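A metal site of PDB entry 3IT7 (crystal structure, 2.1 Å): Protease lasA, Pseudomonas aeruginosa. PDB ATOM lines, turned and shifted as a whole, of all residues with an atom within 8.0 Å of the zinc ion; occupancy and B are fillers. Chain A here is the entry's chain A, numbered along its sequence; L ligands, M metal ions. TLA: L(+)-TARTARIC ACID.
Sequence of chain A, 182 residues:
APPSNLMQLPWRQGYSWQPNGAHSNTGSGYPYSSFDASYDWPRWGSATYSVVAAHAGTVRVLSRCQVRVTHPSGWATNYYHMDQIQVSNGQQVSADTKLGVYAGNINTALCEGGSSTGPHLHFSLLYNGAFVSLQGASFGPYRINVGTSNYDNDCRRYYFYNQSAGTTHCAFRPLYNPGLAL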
ATOM      1  N   ASN A  20       0.383 -11.445  14.043  1.00  0.00           N
ATOM      2  CA  ASN A  20       0.738 -12.800  13.645  1.00  0.00           C
ATOM      3  C   ASN A  20       0.128 -13.836  14.615  1.00  0.00           C
ATOM      4  O   ASN A  20      -0.642 -13.455  15.498  1.00  0.00           O
ATOM      5  CB  ASN A  20       2.262 -12.975  13.448  1.00  0.00           C
ATOM      6  CG  ASN A  20       3.030 -13.010  14.750  1.00  0.00           C
ATOM      7  OD1 ASN A  20       2.463 -12.816  15.815  1.00  0.00           O
ATOM      8  ND2 ASN A  20       4.338 -13.276  14.669  1.00  0.00           N
ATOM      9  N   GLY A  21       0.464 -15.106  14.448  1.00  0.00           N
ATOM     10  CA  GLY A  21      -0.112 -16.177  15.264  1.00  0.00           C
ATOM     11  C   GLY A  21       0.322 -16.151  16.721  1.00  0.00           C
ATOM     12  O   GLY A  21       1.463 -15.807  17.026  1.00  0.00           O
ATOM     13  N   ALA A  22      -0.589 -16.536  17.615  1.00  0.00           N
ATOM     14  CA  ALA A  22      -0.305 -16.589  19.051  1.00  0.00           C
ATOM     15  C   ALA A  22       0.850 -17.539  19.372  1.00  0.00           C
ATOM     16  O   ALA A  22       1.041 -18.552  18.684  1.00  0.00           O
ATOM     17  CB  ALA A  22      -1.535 -17.000  19.831  1.00  0.00           C
ATOM     18  N   HIS A  23       1.602 -17.196  20.418  1.00  0.00           N
ATOM     19  CA  HIS A  23       2.773 -17.966  20.837  1.00  0.00           C
ATOM     20  C   HIS A  23       3.141 -17.659  22.291  1.00  0.00           C
ATOM     21  O   HIS A  23       2.615 -16.716  22.881  1.00  0.00           O
ATOM     22  CB  HIS A  23       3.982 -17.696  19.923  1.00  0.00           C
ATOM     23  CG  HIS A  23       4.269 -16.240  19.697  1.00  0.00           C
ATOM     24  ND1 HIS A  23       3.569 -15.469  18.794  1.00  0.00           N
ATOM     25  CD2 HIS A  23       5.194 -15.415  20.250  1.00  0.00           C
ATOM     26  CE1 HIS A  23       4.043 -14.239  18.795  1.00  0.00           C
ATOM     27  NE2 HIS A  23       5.034 -14.183  19.671  1.00  0.00           N
ATOM     28  N   SER A  24       4.024 -18.476  22.862  1.00  0.00           N
ATOM     29  CA  SER A  24       4.504 -18.235  24.222  1.00  0.00           C
ATOM     30  C   SER A  24       5.499 -17.080  24.217  1.00  0.00           C
ATOM     31  O   SER A  24       5.979 -16.661  23.158  1.00  0.00           O
ATOM     32  CB  SER A  24       5.148 -19.497  24.803  1.00  0.00           C
ATOM     33  OG  SER A  24       6.468 -19.650  24.316  1.00  0.00           O
ATOM     34  N   ASN A  25       5.805 -16.557  25.405  1.00  0.00           N
ATOM     35  CA  ASN A  25       6.747 -15.453  25.532  1.00  0.00           C
ATOM     36  C   ASN A  25       8.130 -15.765  24.951  1.00  0.00           C
ATOM     37  O   ASN A  25       8.750 -14.902  24.324  1.00  0.00           O
ATOM     38  CB  ASN A  25       6.873 -14.979  26.976  1.00  0.00           C
ATOM     39  CG  ASN A  25       7.753 -13.752  27.108  1.00  0.00           C
ATOM     40  OD1 ASN A  25       7.543 -12.737  26.423  1.00  0.00           O
ATOM     41  ND2 ASN A  25       8.766 -13.839  27.984  1.00  0.00           N
ATOM     42  N   THR A  26       8.592 -16.995  25.175  1.00  0.00           N
ATOM     43  CA  THR A  26       9.878 -17.450  24.646  1.00  0.00           C
ATOM     44  C   THR A  26       9.786 -17.794  23.157  1.00  0.00           C
ATOM     45  O   THR A  26      10.792 -17.772  22.442  1.00  0.00           O
ATOM     46  CB  THR A  26      10.399 -18.695  25.397  1.00  0.00           C
ATOM     47  OG1 THR A  26       9.482 -19.782  25.219  1.00  0.00           O
ATOM     48  CG2 THR A  26      10.548 -18.422  26.903  1.00  0.00           C
ATOM     49  N   GLY A  27       8.587 -18.115  22.688  1.00  0.00           N
ATOM     50  CA  GLY A  27       8.389 -18.522  21.296  1.00  0.00           C
ATOM     51  C   GLY A  27       8.446 -20.033  21.073  1.00  0.00           C
ATOM     52  O   GLY A  27       8.194 -20.514  19.963  1.00  0.00           O
ATOM     53  N   SER A  34       1.189 -14.642  23.959  1.00  0.00           N
ATOM     54  CA  SER A  34       1.702 -13.520  23.167  1.00  0.00           C
ATOM     55  C   SER A  34       1.244 -13.526  21.720  1.00  0.00           C
ATOM     56  O   SER A  34       1.047 -14.590  21.113  1.00  0.00           O
ATOM     57  CB  SER A  34       3.240 -13.549  23.174  1.00  0.00           C
ATOM     58  OG  SER A  34       3.772 -13.604  24.482  1.00  0.00           O
ATOM     59  N   PHE A  35       1.082 -12.348  21.146  1.00  0.00           N
ATOM     60  CA  PHE A  35       1.065 -12.204  19.686  1.00  0.00           C
ATOM     61  C   PHE A  35       1.900 -11.013  19.278  1.00  0.00           C
ATOM     62  O   PHE A  35       2.133 -10.112  20.082  1.00  0.00           O
ATOM     63  CB  PHE A  35      -0.366 -12.162  19.101  1.00  0.00           C
ATOM     64  CG  PHE A  35      -1.155 -10.914  19.422  1.00  0.00           C
ATOM     65  CD1 PHE A  35      -1.070  -9.780  18.603  1.00  0.00           C
ATOM     66  CD2 PHE A  35      -2.037 -10.892  20.506  1.00  0.00           C
ATOM     67  CE1 PHE A  35      -1.839  -8.623  18.882  1.00  0.00           C
ATOM     68  CE2 PHE A  35      -2.802  -9.752  20.785  1.00  0.00           C
ATOM     69  CZ  PHE A  35      -2.696  -8.625  19.977  1.00  0.00           C
ATOM     70  N   ASP A  36       2.384 -11.036  18.043  1.00  0.00           N
ATOM     71  CA  ASP A  36       3.177  -9.931  17.521  1.00  0.00           C
ATOM     72  C   ASP A  36       2.297  -9.080  16.626  1.00  0.00           C
ATOM     73  O   ASP A  36       1.328  -9.584  16.047  1.00  0.00           O
ATOM     74  CB  ASP A  36       4.388 -10.433  16.728  1.00  0.00           C
ATOM     75  CG  ASP A  36       5.303 -11.348  17.527  1.00  0.00           C
ATOM     76  OD1 ASP A  36       5.473 -11.136  18.753  1.00  0.00           O
ATOM     77  OD2 ASP A  36       5.875 -12.276  16.926  1.00  0.00           O
ATOM     78  N   ALA A  37       2.627  -7.797  16.496  1.00  0.00           N
ATOM     79  CA  ALA A  37       1.909  -6.948  15.564  1.00  0.00           C
ATOM     80  C   ALA A  37       2.811  -5.915  14.933  1.00  0.00           C
ATOM     81  O   ALA A  37       3.781  -5.463  15.553  1.00  0.00           O
ATOM     82  CB  ALA A  37       0.708  -6.274  16.235  1.00  0.00           C
ATOM     83  N   TRP A  41       4.774  -5.271   8.592  1.00  0.00           N
ATOM     84  CA  TRP A  41       5.804  -6.325   8.672  1.00  0.00           C
ATOM     85  C   TRP A  41       6.962  -6.089   7.695  1.00  0.00           C
ATOM     86  O   TRP A  41       7.230  -6.922   6.821  1.00  0.00           O
ATOM     87  CB  TRP A  41       5.174  -7.729   8.500  1.00  0.00           C
ATOM     88  CG  TRP A  41       4.410  -8.136   9.722  1.00  0.00           C
ATOM     89  CD1 TRP A  41       3.081  -7.944   9.970  1.00  0.00           C
ATOM     90  CD2 TRP A  41       4.948  -8.756  10.900  1.00  0.00           C
ATOM     91  NE1 TRP A  41       2.748  -8.420  11.218  1.00  0.00           N
ATOM     92  CE2 TRP A  41       3.878  -8.933  11.812  1.00  0.00           C
ATOM     93  CE3 TRP A  41       6.226  -9.197  11.269  1.00  0.00           C
ATOM     94  CZ2 TRP A  41       4.054  -9.516  13.065  1.00  0.00           C
ATOM     95  CZ3 TRP A  41       6.404  -9.780  12.508  1.00  0.00           C
ATOM     96  CH2 TRP A  41       5.324  -9.941  13.396  1.00  0.00           C
ATOM     97  N   TYR A  80       7.423  -5.797  24.115  1.00  0.00           N
ATOM     98  CA  TYR A  80       8.833  -6.108  23.830  1.00  0.00           C
ATOM     99  C   TYR A  80       9.242  -5.764  22.383  1.00  0.00           C
ATOM    100  O   TYR A  80       8.393  -5.738  21.483  1.00  0.00           O
ATOM    101  CB  TYR A  80       9.087  -7.581  24.194  1.00  0.00           C
ATOM    102  CG  TYR A  80      10.505  -8.084  23.997  1.00  0.00           C
ATOM    103  CD1 TYR A  80      11.587  -7.462  24.627  1.00  0.00           C
ATOM    104  CD2 TYR A  80      10.758  -9.214  23.217  1.00  0.00           C
ATOM    105  CE1 TYR A  80      12.885  -7.931  24.455  1.00  0.00           C
ATOM    106  CE2 TYR A  80      12.059  -9.700  23.045  1.00  0.00           C
ATOM    107  CZ  TYR A  80      13.111  -9.049  23.669  1.00  0.00           C
ATOM    108  OH  TYR A  80      14.389  -9.528  23.500  1.00  0.00           O
ATOM    109  N   HIS A  81      10.535  -5.521  22.181  1.00  0.00           N
ATOM    110  CA  HIS A  81      11.089  -4.946  20.935  1.00  0.00           C
ATOM    111  C   HIS A  81      10.630  -3.485  20.771  1.00  0.00           C
ATOM    112  O   HIS A  81      10.385  -3.022  19.650  1.00  0.00           O
ATOM    113  CB  HIS A  81      10.688  -5.748  19.670  1.00  0.00           C
ATOM    114  CG  HIS A  81      11.070  -7.190  19.702  1.00  0.00           C
ATOM    115  ND1 HIS A  81      12.345  -7.632  19.969  1.00  0.00           N
ATOM    116  CD2 HIS A  81      10.332  -8.299  19.454  1.00  0.00           C
ATOM    117  CE1 HIS A  81      12.387  -8.945  19.895  1.00  0.00           C
ATOM    118  NE2 HIS A  81      11.174  -9.386  19.585  1.00  0.00           N
ATOM    119  N   SER A 116      15.367 -11.766  15.671  1.00  0.00           N
ATOM    120  CA  SER A 116      14.079 -11.339  15.118  1.00  0.00           C
ATOM    121  C   SER A 116      14.137 -11.127  13.604  1.00  0.00           C
ATOM    122  O   SER A 116      15.201 -10.850  13.043  1.00  0.00           O
ATOM    123  CB  SER A 116      13.602 -10.067  15.812  1.00  0.00           C
ATOM    124  OG  SER A 116      12.355  -9.661  15.304  1.00  0.00           O
ATOM    125  N   HIS A 120       8.547  -5.247  14.692  1.00  0.00           N
ATOM    126  CA  HIS A 120       7.229  -5.588  15.225  1.00  0.00           C
ATOM    127  C   HIS A 120       7.203  -5.445  16.739  1.00  0.00           C
ATOM    128  O   HIS A 120       8.256  -5.460  17.387  1.00  0.00           O
ATOM    129  CB  HIS A 120       6.845  -7.031  14.851  1.00  0.00           C
ATOM    130  CG  HIS A 120       7.682  -8.063  15.520  1.00  0.00           C
ATOM    131  ND1 HIS A 120       8.885  -8.501  15.003  1.00  0.00           N
ATOM    132  CD2 HIS A 120       7.500  -8.762  16.669  1.00  0.00           C
ATOM    133  CE1 HIS A 120       9.407  -9.415  15.804  1.00  0.00           C
ATOM    134  NE2 HIS A 120       8.589  -9.586  16.821  1.00  0.00           N
ATOM    135  N   LEU A 121       6.002  -5.320  17.294  1.00  0.00           N
ATOM    136  CA  LEU A 121       5.783  -5.394  18.728  1.00  0.00           C
ATOM    137  C   LEU A 121       5.548  -6.856  19.132  1.00  0.00           C
ATOM    138  O   LEU A 121       4.819  -7.570  18.459  1.00  0.00           O
ATOM    139  CB  LEU A 121       4.557  -4.562  19.118  1.00  0.00           C
ATOM    140  CG  LEU A 121       4.005  -4.729  20.541  1.00  0.00           C
ATOM    141  CD1 LEU A 121       4.937  -4.071  21.596  1.00  0.00           C
ATOM    142  CD2 LEU A 121       2.587  -4.143  20.626  1.00  0.00           C
ATOM    143  N   HIS A 122       6.179  -7.281  20.229  1.00  0.00           N
ATOM    144  CA  HIS A 122       5.870  -8.568  20.870  1.00  0.00           C
ATOM    145  C   HIS A 122       5.057  -8.248  22.119  1.00  0.00           C
ATOM    146  O   HIS A 122       5.549  -7.599  23.048  1.00  0.00           O
ATOM    147  CB  HIS A 122       7.170  -9.335  21.194  1.00  0.00           C
ATOM    148  CG  HIS A 122       6.976 -10.557  22.044  1.00  0.00           C
ATOM    149  ND1 HIS A 122       6.700 -11.802  21.520  1.00  0.00           N
ATOM    150  CD2 HIS A 122       7.050 -10.725  23.385  1.00  0.00           C
ATOM    151  CE1 HIS A 122       6.606 -12.678  22.500  1.00  0.00           C
ATOM    152  NE2 HIS A 122       6.810 -12.053  23.649  1.00  0.00           N
ATOM    153  N   PHE A 123       3.797  -8.704  22.102  1.00  0.00           N
ATOM    154  CA  PHE A 123       2.803  -8.310  23.096  1.00  0.00           C
ATOM    155  C   PHE A 123       2.330  -9.542  23.849  1.00  0.00           C
ATOM    156  O   PHE A 123       1.996 -10.558  23.221  1.00  0.00           O
ATOM    157  CB  PHE A 123       1.618  -7.632  22.367  1.00  0.00           C
ATOM    158  CG  PHE A 123       0.445  -7.270  23.256  1.00  0.00           C
ATOM    159  CD1 PHE A 123       0.526  -6.212  24.157  1.00  0.00           C
ATOM    160  CD2 PHE A 123      -0.761  -7.957  23.140  1.00  0.00           C
ATOM    161  CE1 PHE A 123      -0.573  -5.858  24.968  1.00  0.00           C
ATOM    162  CE2 PHE A 123      -1.869  -7.605  23.942  1.00  0.00           C
ATOM    163  CZ  PHE A 123      -1.765  -6.559  24.862  1.00  0.00           C
ATOM    164  N   SER A 124       2.291  -9.468  25.183  1.00  0.00           N
ATOM    165  CA  SER A 124       1.983 -10.624  26.025  1.00  0.00           C
ATOM    166  C   SER A 124       0.969 -10.322  27.135  1.00  0.00           C
ATOM    167  O   SER A 124       0.930  -9.202  27.657  1.00  0.00           O
ATOM    168  CB  SER A 124       3.251 -11.178  26.669  1.00  0.00           C
ATOM    169  OG  SER A 124       4.245 -11.484  25.707  1.00  0.00           O
ATOM    170  N   TYR A 151       3.092 -19.715  17.048  1.00  0.00           N
ATOM    171  CA  TYR A 151       2.984 -18.959  15.788  1.00  0.00           C
ATOM    172  C   TYR A 151       1.995 -19.545  14.767  1.00  0.00           C
ATOM    173  O   TYR A 151       1.946 -19.077  13.624  1.00  0.00           O
ATOM    174  CB  TYR A 151       4.373 -18.738  15.142  1.00  0.00           C
ATOM    175  CG  TYR A 151       5.355 -18.053  16.064  1.00  0.00           C
ATOM    176  CD1 TYR A 151       6.248 -18.791  16.837  1.00  0.00           C
ATOM    177  CD2 TYR A 151       5.396 -16.659  16.166  1.00  0.00           C
ATOM    178  CE1 TYR A 151       7.149 -18.170  17.702  1.00  0.00           C
ATOM    179  CE2 TYR A 151       6.303 -16.013  17.019  1.00  0.00           C
ATOM    180  CZ  TYR A 151       7.180 -16.789  17.787  1.00  0.00           C
ATOM    181  OH  TYR A 151       8.081 -16.180  18.644  1.00  0.00           O
HETATM  182  O1  TLA L   1       8.130 -13.526  19.197  1.00  0.00           O
HETATM  183  O11 TLA L   1       8.494 -11.388  18.922  1.00  0.00           O
HETATM  184  C1  TLA L   1       8.799 -12.594  18.722  1.00  0.00           C
HETATM  185  C2  TLA L   1      10.017 -12.929  17.893  1.00  0.00           C
HETATM  186  O2  TLA L   1      10.781 -11.764  17.578  1.00  0.00           O
HETATM  187  C3  TLA L   1       9.582 -13.597  16.592  1.00  0.00           C
HETATM  188  O3  TLA L   1       8.762 -12.709  15.834  1.00  0.00           O
HETATM  189  C4  TLA L   1      10.828 -13.943  15.820  1.00  0.00           C
HETATM  190  O4  TLA L   1      11.626 -14.766  16.336  1.00  0.00           O
HETATM  191  O41 TLA L   1      11.019 -13.384  14.704  1.00  0.00           O
HETATM  192 ZN    ZN M   1       6.361 -12.528  19.701  1.00  0.00          ZN
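The backbone NH (N) of Asp 36 lies within hydrogen-bond range of the side-chain amide oxygen (OD1) of Asn 20 (2.9 Å).
NE2 of His 122 is in hydrogen-bond range of OD1 of Asn 25 (2.9 Å).
NE2 of His 122 sits at hydrogen-bond distance from OG of Ser 124, at 3.3 Å.
The backbone carbonyl oxygen (O) of His 122 lies within hydrogen-bond range of the backbone NH (N) of Tyr 80.
The backbone NH (N) of Ser 34 is in hydrogen-bond range of the backbone carbonyl oxygen (O) of His 23, at 2.7 Å.
O of Gly 21 lies within hydrogen-bond range of ND1 of His 23, at 2.8 Å.
Within 4 Å of the zinc ion: His 23, Asp 36 and His 122.
The nearest printed residue that does not touch the zinc ion is Tyr 151 (4.2 Å).
The zinc ion is bound by the side-chain carboxylate (OD1) of Asp 36, a ring nitrogen (ND1) of His 122, an oxygen (O1) of the ligand, a ring nitrogen (NE2) of His 23 and an oxygen (O11) of the ligand.
The zinc ion has five donor atoms within binding distance.
Slightly farther from the zinc ion lies OD2 of Asp 36 (2.8 Å).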
